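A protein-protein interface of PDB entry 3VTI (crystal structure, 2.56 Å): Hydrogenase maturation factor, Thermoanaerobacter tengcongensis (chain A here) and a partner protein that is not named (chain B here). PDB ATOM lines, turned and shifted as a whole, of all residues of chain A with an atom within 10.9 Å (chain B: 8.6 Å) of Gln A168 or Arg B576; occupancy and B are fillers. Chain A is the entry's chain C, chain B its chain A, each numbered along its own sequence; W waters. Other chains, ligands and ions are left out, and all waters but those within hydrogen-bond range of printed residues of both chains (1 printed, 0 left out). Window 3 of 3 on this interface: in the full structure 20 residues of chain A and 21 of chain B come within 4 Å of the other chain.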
ATOM      1  N   PRO A  45      21.249 -21.962  -0.375  1.00  0.00           N
ATOM      2  CA  PRO A  45      21.555 -20.685   0.265  1.00  0.00           C
ATOM      3  C   PRO A  45      22.535 -20.847   1.435  1.00  0.00           C
ATOM      4  O   PRO A  45      22.319 -21.677   2.326  1.00  0.00           O
ATOM      5  CB  PRO A  45      20.186 -20.219   0.757  1.00  0.00           C
ATOM      6  CG  PRO A  45      19.239 -20.773  -0.257  1.00  0.00           C
ATOM      7  CD  PRO A  45      19.797 -22.140  -0.568  1.00  0.00           C
ATOM      8  N   MET A 158      16.473 -26.173   8.034  1.00  0.00           N
ATOM      9  CA  MET A 158      15.388 -25.471   7.372  1.00  0.00           C
ATOM     10  C   MET A 158      15.808 -24.912   6.012  1.00  0.00           C
ATOM     11  O   MET A 158      15.002 -24.857   5.092  1.00  0.00           O
ATOM     12  CB  MET A 158      14.788 -24.388   8.270  1.00  0.00           C
ATOM     13  CG  MET A 158      13.492 -23.778   7.732  1.00  0.00           C
ATOM     14  SD  MET A 158      12.223 -24.974   7.212  1.00  0.00           S
ATOM     15  CE  MET A 158      11.585 -25.510   8.798  1.00  0.00           C
ATOM     16  N   ALA A 159      17.070 -24.522   5.881  1.00  0.00           N
ATOM     17  CA  ALA A 159      17.568 -23.961   4.626  1.00  0.00           C
ATOM     18  C   ALA A 159      17.542 -24.969   3.477  1.00  0.00           C
ATOM     19  O   ALA A 159      17.004 -24.669   2.409  1.00  0.00           O
ATOM     20  CB  ALA A 159      18.976 -23.362   4.805  1.00  0.00           C
ATOM     21  N   VAL A 160      18.105 -26.158   3.690  1.00  0.00           N
ATOM     22  CA  VAL A 160      18.113 -27.174   2.634  1.00  0.00           C
ATOM     23  C   VAL A 160      16.708 -27.727   2.376  1.00  0.00           C
ATOM     24  O   VAL A 160      16.353 -27.971   1.234  1.00  0.00           O
ATOM     25  CB  VAL A 160      19.196 -28.294   2.826  1.00  0.00           C
ATOM     26  CG1 VAL A 160      20.436 -27.743   3.518  1.00  0.00           C
ATOM     27  CG2 VAL A 160      18.651 -29.500   3.575  1.00  0.00           C
ATOM     28  N   MET A 161      15.909 -27.886   3.429  1.00  0.00           N
ATOM     29  CA  MET A 161      14.479 -28.204   3.306  1.00  0.00           C
ATOM     30  C   MET A 161      13.769 -27.236   2.347  1.00  0.00           C
ATOM     31  O   MET A 161      13.082 -27.658   1.419  1.00  0.00           O
ATOM     32  CB  MET A 161      13.825 -28.162   4.696  1.00  0.00           C
ATOM     33  CG  MET A 161      12.299 -28.132   4.730  1.00  0.00           C
ATOM     34  SD  MET A 161      11.536 -29.625   5.396  1.00  0.00           S
ATOM     35  CE  MET A 161      12.030 -29.570   7.115  1.00  0.00           C
ATOM     36  N   SER A 162      13.961 -25.941   2.580  1.00  0.00           N
ATOM     37  CA  SER A 162      13.348 -24.882   1.788  1.00  0.00           C
ATOM     38  C   SER A 162      13.766 -24.927   0.317  1.00  0.00           C
ATOM     39  O   SER A 162      12.934 -24.776  -0.577  1.00  0.00           O
ATOM     40  CB  SER A 162      13.695 -23.518   2.384  1.00  0.00           C
ATOM     41  OG  SER A 162      13.204 -22.478   1.564  1.00  0.00           O
ATOM     42  N   ALA A 163      15.058 -25.128   0.080  1.00  0.00           N
ATOM     43  CA  ALA A 163      15.583 -25.211  -1.271  1.00  0.00           C
ATOM     44  C   ALA A 163      15.196 -26.523  -1.955  1.00  0.00           C
ATOM     45  O   ALA A 163      14.817 -26.519  -3.118  1.00  0.00           O
ATOM     46  CB  ALA A 163      17.096 -25.031  -1.255  1.00  0.00           C
ATOM     47  N   ARG A 164      15.283 -27.633  -1.226  1.00  0.00           N
ATOM     48  CA  ARG A 164      15.046 -28.974  -1.773  1.00  0.00           C
ATOM     49  C   ARG A 164      13.588 -29.222  -2.109  1.00  0.00           C
ATOM     50  O   ARG A 164      13.281 -29.871  -3.107  1.00  0.00           O
ATOM     51  CB  ARG A 164      15.541 -30.050  -0.796  1.00  0.00           C
ATOM     52  CG  ARG A 164      15.333 -31.513  -1.227  1.00  0.00           C
ATOM     53  CD  ARG A 164      15.713 -32.468  -0.082  1.00  0.00           C
ATOM     54  NE  ARG A 164      14.683 -32.510   0.964  1.00  0.00           N
ATOM     55  CZ  ARG A 164      14.919 -32.518   2.276  1.00  0.00           C
ATOM     56  NH1 ARG A 164      13.895 -32.551   3.129  1.00  0.00           N
ATOM     57  NH2 ARG A 164      16.164 -32.472   2.744  1.00  0.00           N
ATOM     58  N   GLU A 165      12.693 -28.708  -1.269  1.00  0.00           N
ATOM     59  CA  GLU A 165      11.264 -28.933  -1.441  1.00  0.00           C
ATOM     60  C   GLU A 165      10.535 -27.715  -1.996  1.00  0.00           C
ATOM     61  O   GLU A 165       9.300 -27.680  -1.997  1.00  0.00           O
ATOM     62  CB  GLU A 165      10.630 -29.403  -0.126  1.00  0.00           C
ATOM     63  CG  GLU A 165      11.252 -30.665   0.465  1.00  0.00           C
ATOM     64  CD  GLU A 165      11.153 -31.894  -0.444  1.00  0.00           C
ATOM     65  OE1 GLU A 165      10.270 -31.934  -1.339  1.00  0.00           O
ATOM     66  OE2 GLU A 165      11.973 -32.828  -0.255  1.00  0.00           O
ATOM     67  N   GLU A 166      11.307 -26.734  -2.471  1.00  0.00           N
ATOM     68  CA  GLU A 166      10.787 -25.536  -3.155  1.00  0.00           C
ATOM     69  C   GLU A 166       9.782 -24.741  -2.326  1.00  0.00           C
ATOM     70  O   GLU A 166       8.879 -24.112  -2.861  1.00  0.00           O
ATOM     71  CB  GLU A 166      10.203 -25.896  -4.530  1.00  0.00           C
ATOM     72  CG  GLU A 166      11.250 -26.024  -5.613  1.00  0.00           C
ATOM     73  CD  GLU A 166      10.845 -26.970  -6.724  1.00  0.00           C
ATOM     74  OE1 GLU A 166       9.817 -26.721  -7.407  1.00  0.00           O
ATOM     75  OE2 GLU A 166      11.578 -27.963  -6.923  1.00  0.00           O
ATOM     76  N   LEU A 167       9.966 -24.770  -1.014  1.00  0.00           N
ATOM     77  CA  LEU A 167       9.101 -24.066  -0.085  1.00  0.00           C
ATOM     78  C   LEU A 167       9.504 -22.603   0.007  1.00  0.00           C
ATOM     79  O   LEU A 167      10.591 -22.271   0.490  1.00  0.00           O
ATOM     80  CB  LEU A 167       9.174 -24.718   1.301  1.00  0.00           C
ATOM     81  CG  LEU A 167       9.009 -26.238   1.391  1.00  0.00           C
ATOM     82  CD1 LEU A 167       9.398 -26.719   2.767  1.00  0.00           C
ATOM     83  CD2 LEU A 167       7.592 -26.654   1.065  1.00  0.00           C
ATOM     84  N   GLN A 168       8.626 -21.731  -0.472  1.00  0.00           N
ATOM     85  CA  GLN A 168       8.854 -20.291  -0.393  1.00  0.00           C
ATOM     86  C   GLN A 168       8.442 -19.774   0.982  1.00  0.00           C
ATOM     87  O   GLN A 168       7.368 -20.110   1.485  1.00  0.00           O
ATOM     88  CB  GLN A 168       8.090 -19.561  -1.511  1.00  0.00           C
ATOM     89  CG  GLN A 168       8.253 -18.034  -1.523  1.00  0.00           C
ATOM     90  CD  GLN A 168       9.682 -17.582  -1.792  1.00  0.00           C
ATOM     91  OE1 GLN A 168      10.151 -17.610  -2.934  1.00  0.00           O
ATOM     92  NE2 GLN A 168      10.374 -17.145  -0.742  1.00  0.00           N
ATOM     93  N   PHE A 169       9.314 -18.980   1.597  1.00  0.00           N
ATOM     94  CA  PHE A 169       8.999 -18.337   2.874  1.00  0.00           C
ATOM     95  C   PHE A 169       9.057 -16.820   2.751  1.00  0.00           C
ATOM     96  O   PHE A 169       9.636 -16.286   1.802  1.00  0.00           O
ATOM     97  CB  PHE A 169       9.934 -18.822   3.982  1.00  0.00           C
ATOM     98  CG  PHE A 169       9.783 -20.280   4.309  1.00  0.00           C
ATOM     99  CD1 PHE A 169       8.551 -20.796   4.703  1.00  0.00           C
ATOM    100  CD2 PHE A 169      10.875 -21.137   4.239  1.00  0.00           C
ATOM    101  CE1 PHE A 169       8.414 -22.150   5.009  1.00  0.00           C
ATOM    102  CE2 PHE A 169      10.746 -22.489   4.548  1.00  0.00           C
ATOM    103  CZ  PHE A 169       9.516 -22.996   4.931  1.00  0.00           C
ATOM    104  N   ASP A 170       8.452 -16.137   3.719  1.00  0.00           N
ATOM    105  CA  ASP A 170       8.450 -14.677   3.768  1.00  0.00           C
ATOM    106  C   ASP A 170       9.877 -14.124   3.844  1.00  0.00           C
ATOM    107  O   ASP A 170      10.167 -13.061   3.290  1.00  0.00           O
ATOM    108  CB  ASP A 170       7.600 -14.186   4.947  1.00  0.00           C
ATOM    109  CG  ASP A 170       6.128 -14.590   4.824  1.00  0.00           C
ATOM    110  OD1 ASP A 170       5.527 -15.005   5.846  1.00  0.00           O
ATOM    111  OD2 ASP A 170       5.577 -14.491   3.701  1.00  0.00           O
ATOM    112  N   THR A 171      10.753 -14.866   4.522  1.00  0.00           N
ATOM    113  CA  THR A 171      12.181 -14.561   4.595  1.00  0.00           C
ATOM    114  C   THR A 171      13.001 -15.766   4.080  1.00  0.00           C
ATOM    115  O   THR A 171      12.797 -16.898   4.540  1.00  0.00           O
ATOM    116  CB  THR A 171      12.608 -14.240   6.054  1.00  0.00           C
ATOM    117  OG1 THR A 171      11.522 -13.617   6.749  1.00  0.00           O
ATOM    118  CG2 THR A 171      13.836 -13.327   6.089  1.00  0.00           C
ATOM    119  N   PRO A 172      13.923 -15.535   3.123  1.00  0.00           N
ATOM    120  CA  PRO A 172      14.806 -16.636   2.729  1.00  0.00           C
ATOM    121  C   PRO A 172      15.689 -17.074   3.906  1.00  0.00           C
ATOM    122  O   PRO A 172      16.149 -16.236   4.696  1.00  0.00           O
ATOM    123  CB  PRO A 172      15.651 -16.031   1.599  1.00  0.00           C
ATOM    124  CG  PRO A 172      15.564 -14.551   1.795  1.00  0.00           C
ATOM    125  CD  PRO A 172      14.205 -14.299   2.370  1.00  0.00           C
ATOM    126  N   ILE A 173      15.889 -18.384   4.027  1.00  0.00           N
ATOM    127  CA  ILE A 173      16.685 -18.957   5.100  1.00  0.00           C
ATOM    128  C   ILE A 173      18.005 -19.461   4.538  1.00  0.00           C
ATOM    129  O   ILE A 173      18.027 -20.184   3.539  1.00  0.00           O
ATOM    130  CB  ILE A 173      15.917 -20.076   5.854  1.00  0.00           C
ATOM    131  CG1 ILE A 173      14.805 -19.454   6.698  1.00  0.00           C
ATOM    132  CG2 ILE A 173      16.847 -20.864   6.771  1.00  0.00           C
ATOM    133  CD1 ILE A 173      13.592 -20.317   6.879  1.00  0.00           C
ATOM    134  N   PHE A 174      19.092 -19.056   5.188  1.00  0.00           N
ATOM    135  CA  PHE A 174      20.442 -19.442   4.799  1.00  0.00           C
ATOM    136  C   PHE A 174      21.007 -20.484   5.742  1.00  0.00           C
ATOM    137  O   PHE A 174      20.728 -20.473   6.940  1.00  0.00           O
ATOM    138  CB  PHE A 174      21.356 -18.220   4.786  1.00  0.00           C
ATOM    139  CG  PHE A 174      21.026 -17.237   3.705  1.00  0.00           C
ATOM    140  CD1 PHE A 174      20.027 -16.281   3.893  1.00  0.00           C
ATOM    141  CD2 PHE A 174      21.705 -17.273   2.485  1.00  0.00           C
ATOM    142  CE1 PHE A 174      19.716 -15.375   2.882  1.00  0.00           C
ATOM    143  CE2 PHE A 174      21.400 -16.370   1.463  1.00  0.00           C
ATOM    144  CZ  PHE A 174      20.408 -15.420   1.663  1.00  0.00           C
ATOM    145  N   SER A 232      12.951 -16.169  11.076  1.00  0.00           N
ATOM    146  CA  SER A 232      12.637 -16.856   9.831  1.00  0.00           C
ATOM    147  C   SER A 232      12.478 -18.363  10.057  1.00  0.00           C
ATOM    148  O   SER A 232      11.558 -18.982   9.518  1.00  0.00           O
ATOM    149  CB  SER A 232      13.703 -16.570   8.777  1.00  0.00           C
ATOM    150  OG  SER A 232      14.969 -17.013   9.208  1.00  0.00           O
ATOM    151  N   SER A 235       9.085 -19.077  12.458  1.00  0.00           N
ATOM    152  CA  SER A 235       7.784 -19.098  11.787  1.00  0.00           C
ATOM    153  C   SER A 235       7.683 -20.130  10.651  1.00  0.00           C
ATOM    154  O   SER A 235       6.592 -20.612  10.354  1.00  0.00           O
ATOM    155  CB  SER A 235       7.369 -17.694  11.322  1.00  0.00           C
ATOM    156  OG  SER A 235       8.188 -17.226  10.279  1.00  0.00           O
ATOM    157  N   ALA A 236       8.811 -20.469  10.030  1.00  0.00           N
ATOM    158  CA  ALA A 236       8.843 -21.537   9.036  1.00  0.00           C
ATOM    159  C   ALA A 236       8.425 -22.865   9.674  1.00  0.00           C
ATOM    160  O   ALA A 236       7.594 -23.603   9.118  1.00  0.00           O
ATOM    161  CB  ALA A 236      10.219 -21.650   8.422  1.00  0.00           C
ATOM    162  N   CYS A 237       9.006 -23.150  10.843  1.00  0.00           N
ATOM    163  CA  CYS A 237       8.670 -24.320  11.645  1.00  0.00           C
ATOM    164  C   CYS A 237       7.245 -24.242  12.199  1.00  0.00           C
ATOM    165  O   CYS A 237       6.551 -25.251  12.261  1.00  0.00           O
ATOM    166  CB  CYS A 237       9.665 -24.477  12.803  1.00  0.00           C
ATOM    167  SG  CYS A 237      11.377 -24.894  12.329  1.00  0.00           S
ATOM    168  N   GLU A 238       6.822 -23.047  12.607  1.00  0.00           N
ATOM    169  CA  GLU A 238       5.497 -22.847  13.192  1.00  0.00           C
ATOM    170  C   GLU A 238       4.405 -23.028  12.136  1.00  0.00           C
ATOM    171  O   GLU A 238       3.255 -23.335  12.458  1.00  0.00           O
ATOM    172  CB  GLU A 238       5.398 -21.461  13.833  1.00  0.00           C
ATOM    173  CG  GLU A 238       4.489 -21.395  15.052  1.00  0.00           C
ATOM    174  CD  GLU A 238       3.012 -21.323  14.694  1.00  0.00           C
ATOM    175  OE1 GLU A 238       2.197 -21.919  15.425  1.00  0.00           O
ATOM    176  OE2 GLU A 238       2.665 -20.676  13.683  1.00  0.00           O
ATOM    177  N   PHE A 239       4.770 -22.837  10.873  1.00  0.00           N
ATOM    178  CA  PHE A 239       3.834 -23.007   9.778  1.00  0.00           C
ATOM    179  C   PHE A 239       3.626 -24.463   9.422  1.00  0.00           C
ATOM    180  O   PHE A 239       2.581 -24.823   8.904  1.00  0.00           O
ATOM    181  CB  PHE A 239       4.306 -22.245   8.547  1.00  0.00           C
ATOM    182  CG  PHE A 239       3.960 -20.788   8.568  1.00  0.00           C
ATOM    183  CD1 PHE A 239       2.972 -20.306   9.420  1.00  0.00           C
ATOM    184  CD2 PHE A 239       4.608 -19.903   7.713  1.00  0.00           C
ATOM    185  CE1 PHE A 239       2.642 -18.962   9.434  1.00  0.00           C
ATOM    186  CE2 PHE A 239       4.288 -18.555   7.712  1.00  0.00           C
ATOM    187  CZ  PHE A 239       3.299 -18.080   8.576  1.00  0.00           C
ATOM    188  N   MET A 240       4.627 -25.289   9.704  1.00  0.00           N
ATOM    189  CA  MET A 240       4.596 -26.702   9.357  1.00  0.00           C
ATOM    190  C   MET A 240       4.476 -27.580  10.590  1.00  0.00           C
ATOM    191  O   MET A 240       4.458 -28.807  10.478  1.00  0.00           O
ATOM    192  CB  MET A 240       5.857 -27.094   8.593  1.00  0.00           C
ATOM    193  CG  MET A 240       6.033 -26.405   7.258  1.00  0.00           C
ATOM    194  SD  MET A 240       7.628 -26.804   6.541  1.00  0.00           S
ATOM    195  CE  MET A 240       7.277 -28.437   5.903  1.00  0.00           C
ATOM    196  N   VAL B 573      -7.792 -17.999   6.070  1.00  0.00           N
ATOM    197  CA  VAL B 573      -6.437 -18.438   6.426  1.00  0.00           C
ATOM    198  C   VAL B 573      -5.394 -17.567   5.734  1.00  0.00           C
ATOM    199  O   VAL B 573      -5.556 -17.205   4.571  1.00  0.00           O
ATOM    200  CB  VAL B 573      -6.205 -19.940   6.075  1.00  0.00           C
ATOM    201  CG1 VAL B 573      -4.734 -20.331   6.210  1.00  0.00           C
ATOM    202  CG2 VAL B 573      -7.065 -20.833   6.948  1.00  0.00           C
ATOM    203  N   ASP B 574      -4.333 -17.232   6.465  1.00  0.00           N
ATOM    204  CA  ASP B 574      -3.215 -16.464   5.921  1.00  0.00           C
ATOM    205  C   ASP B 574      -2.653 -17.184   4.698  1.00  0.00           C
ATOM    206  O   ASP B 574      -2.423 -18.395   4.722  1.00  0.00           O
ATOM    207  CB  ASP B 574      -2.146 -16.220   7.000  1.00  0.00           C
ATOM    208  CG  ASP B 574      -0.828 -15.744   6.427  1.00  0.00           C
ATOM    209  OD1 ASP B 574       0.017 -16.604   6.105  1.00  0.00           O
ATOM    210  OD2 ASP B 574      -0.630 -14.513   6.310  1.00  0.00           O
ATOM    211  N   SER B 575      -2.461 -16.426   3.627  1.00  0.00           N
ATOM    212  CA  SER B 575      -2.135 -16.990   2.327  1.00  0.00           C
ATOM    213  C   SER B 575      -0.805 -17.721   2.327  1.00  0.00           C
ATOM    214  O   SER B 575      -0.681 -18.789   1.734  1.00  0.00           O
ATOM    215  CB  SER B 575      -2.135 -15.891   1.270  1.00  0.00           C
ATOM    216  OG  SER B 575      -3.287 -15.084   1.409  1.00  0.00           O
ATOM    217  N   ARG B 576       0.185 -17.137   2.993  1.00  0.00           N
ATOM    218  CA  ARG B 576       1.498 -17.748   3.091  1.00  0.00           C
ATOM    219  C   ARG B 576       1.400 -19.079   3.812  1.00  0.00           C
ATOM    220  O   ARG B 576       1.954 -20.074   3.353  1.00  0.00           O
ATOM    221  CB  ARG B 576       2.490 -16.825   3.807  1.00  0.00           C
ATOM    222  CG  ARG B 576       3.939 -17.322   3.764  1.00  0.00           C
ATOM    223  CD  ARG B 576       4.445 -17.515   2.320  1.00  0.00           C
ATOM    224  NE  ARG B 576       4.884 -16.263   1.703  1.00  0.00           N
ATOM    225  CZ  ARG B 576       5.209 -16.127   0.418  1.00  0.00           C
ATOM    226  NH1 ARG B 576       5.135 -17.171  -0.405  1.00  0.00           N
ATOM    227  NH2 ARG B 576       5.601 -14.944  -0.053  1.00  0.00           N
ATOM    228  N   GLU B 577       0.676 -19.085   4.932  1.00  0.00           N
ATOM    229  CA  GLU B 577       0.487 -20.287   5.728  1.00  0.00           C
ATOM    230  C   GLU B 577      -0.225 -21.368   4.923  1.00  0.00           C
ATOM    231  O   GLU B 577       0.203 -22.523   4.921  1.00  0.00           O
ATOM    232  CB  GLU B 577      -0.276 -19.983   7.021  1.00  0.00           C
ATOM    233  CG  GLU B 577      -0.262 -21.155   8.018  1.00  0.00           C
ATOM    234  CD  GLU B 577      -1.073 -20.904   9.269  1.00  0.00           C
ATOM    235  OE1 GLU B 577      -1.643 -19.806   9.416  1.00  0.00           O
ATOM    236  OE2 GLU B 577      -1.143 -21.818  10.115  1.00  0.00           O
ATOM    237  N   LEU B 578      -1.298 -20.981   4.233  1.00  0.00           N
ATOM    238  CA  LEU B 578      -2.075 -21.905   3.403  1.00  0.00           C
ATOM    239  C   LEU B 578      -1.220 -22.593   2.336  1.00  0.00           C
ATOM    240  O   LEU B 578      -1.335 -23.808   2.128  1.00  0.00           O
ATOM    241  CB  LEU B 578      -3.255 -21.177   2.750  1.00  0.00           C
ATOM    242  CG  LEU B 578      -4.181 -21.987   1.838  1.00  0.00           C
ATOM    243  CD1 LEU B 578      -4.919 -23.092   2.601  1.00  0.00           C
ATOM    244  CD2 LEU B 578      -5.163 -21.065   1.130  1.00  0.00           C
ATOM    245  N   ASP B 579      -0.367 -21.807   1.678  1.00  0.00           N
ATOM    246  CA  ASP B 579       0.538 -22.299   0.634  1.00  0.00           C
ATOM    247  C   ASP B 579       1.491 -23.343   1.209  1.00  0.00           C
ATOM    248  O   ASP B 579       1.716 -24.392   0.614  1.00  0.00           O
ATOM    249  CB  ASP B 579       1.321 -21.128   0.033  1.00  0.00           C
ATOM    250  CG  ASP B 579       2.173 -21.527  -1.173  1.00  0.00           C
ATOM    251  OD1 ASP B 579       1.625 -22.077  -2.162  1.00  0.00           O
ATOM    252  OD2 ASP B 579       3.398 -21.259  -1.140  1.00  0.00           O
ATOM    253  N   ILE B 580       2.013 -23.057   2.394  1.00  0.00           N
ATOM    254  CA  ILE B 580       2.980 -23.915   3.043  1.00  0.00           C
ATOM    255  C   ILE B 580       2.297 -25.153   3.618  1.00  0.00           C
ATOM    256  O   ILE B 580       2.847 -26.255   3.547  1.00  0.00           O
ATOM    257  CB  ILE B 580       3.773 -23.120   4.106  1.00  0.00           C
ATOM    258  CG1 ILE B 580       4.777 -22.191   3.411  1.00  0.00           C
ATOM    259  CG2 ILE B 580       4.503 -24.037   5.071  1.00  0.00           C
ATOM    260  CD1 ILE B 580       5.027 -20.897   4.161  1.00  0.00           C
ATOM    261  N   ILE B 581       1.094 -24.977   4.160  1.00  0.00           N
ATOM    262  CA  ILE B 581       0.307 -26.108   4.657  1.00  0.00           C
ATOM    263  C   ILE B 581      -0.007 -27.066   3.519  1.00  0.00           C
ATOM    264  O   ILE B 581       0.187 -28.268   3.651  1.00  0.00           O
ATOM    265  CB  ILE B 581      -0.975 -25.662   5.410  1.00  0.00           C
ATOM    266  CG1 ILE B 581      -0.610 -25.086   6.781  1.00  0.00           C
ATOM    267  CG2 ILE B 581      -1.921 -26.827   5.623  1.00  0.00           C
ATOM    268  CD1 ILE B 581      -1.788 -24.542   7.564  1.00  0.00           C
ATOM    269  N   LEU B 582      -0.456 -26.522   2.389  1.00  0.00           N
ATOM    270  CA  LEU B 582      -0.788 -27.331   1.219  1.00  0.00           C
ATOM    271  C   LEU B 582       0.426 -27.974   0.549  1.00  0.00           C
ATOM    272  O   LEU B 582       0.332 -29.079   0.012  1.00  0.00           O
ATOM    273  CB  LEU B 582      -1.585 -26.510   0.203  1.00  0.00           C
ATOM    274  CG  LEU B 582      -3.048 -26.223   0.547  1.00  0.00           C
ATOM    275  CD1 LEU B 582      -3.712 -25.457  -0.583  1.00  0.00           C
ATOM    276  CD2 LEU B 582      -3.812 -27.513   0.853  1.00  0.00           C
ATOM    277  N   LYS B 583       1.560 -27.283   0.580  1.00  0.00           N
ATOM    278  CA  LYS B 583       2.800 -27.848   0.059  1.00  0.00           C
ATOM    279  C   LYS B 583       3.354 -28.976   0.943  1.00  0.00           C
ATOM    280  O   LYS B 583       3.813 -29.991   0.426  1.00  0.00           O
ATOM    281  CB  LYS B 583       3.844 -26.758  -0.165  1.00  0.00           C
ATOM    282  CG  LYS B 583       3.633 -25.941  -1.437  1.00  0.00           C
ATOM    283  CD  LYS B 583       4.687 -24.833  -1.545  1.00  0.00           C
ATOM    284  CE  LYS B 583       4.391 -23.846  -2.669  1.00  0.00           C
ATOM    285  NZ  LYS B 583       4.853 -24.323  -3.989  1.00  0.00           N
ATOM    286  N   ARG B 587       4.366 -32.732  -0.152  1.00  0.00           N
ATOM    287  CA  ARG B 587       5.731 -33.235  -0.021  1.00  0.00           C
ATOM    288  C   ARG B 587       5.879 -34.234   1.130  1.00  0.00           C
ATOM    289  O   ARG B 587       6.968 -34.761   1.370  1.00  0.00           O
ATOM    290  CB  ARG B 587       6.729 -32.078   0.105  1.00  0.00           C
ATOM    291  CG  ARG B 587       7.158 -31.500  -1.237  1.00  0.00           C
ATOM    292  CD  ARG B 587       6.364 -30.267  -1.640  1.00  0.00           C
ATOM    293  NE  ARG B 587       6.638 -29.902  -3.032  1.00  0.00           N
ATOM    294  CZ  ARG B 587       6.679 -28.657  -3.510  1.00  0.00           C
ATOM    295  NH1 ARG B 587       6.475 -27.610  -2.711  1.00  0.00           N
ATOM    296  NH2 ARG B 587       6.940 -28.455  -4.799  1.00  0.00           N
HETATM  297  O   HOH W   1      -0.196 -23.100  12.142  1.00  0.00           O
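N of Arg B576 sits at hydrogen-bond distance from OD1 of Asp B574 (3.2 Å). The backbone NH (N) of Glu B577 lies within hydrogen-bond range of the side-chain carboxylate (OD1) of Asp B574, 2.8 Å away. The backbone carbonyl oxygen (O) of Leu A167 is in hydrogen-bond range of the side-chain hydroxyl (OG) of Ser A162. NE of Arg A164 is in salt-bridge range of OE2 of Glu A165.
CB of Lys B583 touches CD2 of Leu A167, 3.9 Å away. Arg B576 touches Gln A168 (NH1 to CG, 3.4 Å). Gln A168 touches Ile B580. Phe A169 touches Ile B580 (CD1 to CD1, 3.6 Å). CD1 of Phe A239 touches CG of Glu B577 (3.6 Å). Ile B580 touches Phe A239 (CD1 to CD2, 3.7 Å). Ile B581 touches Phe A239 (CG1 to O, 3.8 Å). Met A240 touches Ile B580 (CG to CG2, 3.6 Å).
Of chain A, only Gln A168 (3.4 Å) and Asp A170 (2.8 Å) come within 4 Å of Arg B576. No residue of chain A comes within 4 Å of Ser B575. No residue of chain A comes within 4 Å of Asp B579. Ile B580 touches just these residues of chain A: Gln A168, Phe A169, Phe A239 and Met A240. Of the printed residues of chain B, Leu A167 touches Lys B583. Of the printed residues of chain A, Glu B577 touches Phe A239 (3.6 Å). Of the printed residues of chain B, Phe A169 touches Ile B580 (3.6 Å). Of the printed residues of chain B, Met A240 touches Ile B580 (3.6 Å). Arg A164 touches none of the printed residues of chain B. Val A160 touches none of the printed residues of chain B. The nearest residue of chain B that does not touch Gln A168 is Asp B579 (4.9 Å). The nearest printed residue of chain B that does not touch Leu A167 is Arg B587 (4.1 Å).
Of the 12 printed residues of chain B, 6 touch a printed residue of chain A. Hydrophobic or aromatic side chains of chain B that line the printed part of chain A: Ile B580 and Ile B581.
Water W1 bridges OE2 of Glu B577 (2.6 Å) and O of Glu A238 (3.5 Å).
NH1 of Arg B587 sits at hydrogen-bond distance from O of Glu A165. NE of Arg B576 is in salt-bridge range of OD2 of Asp A170 (2.8 Å).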
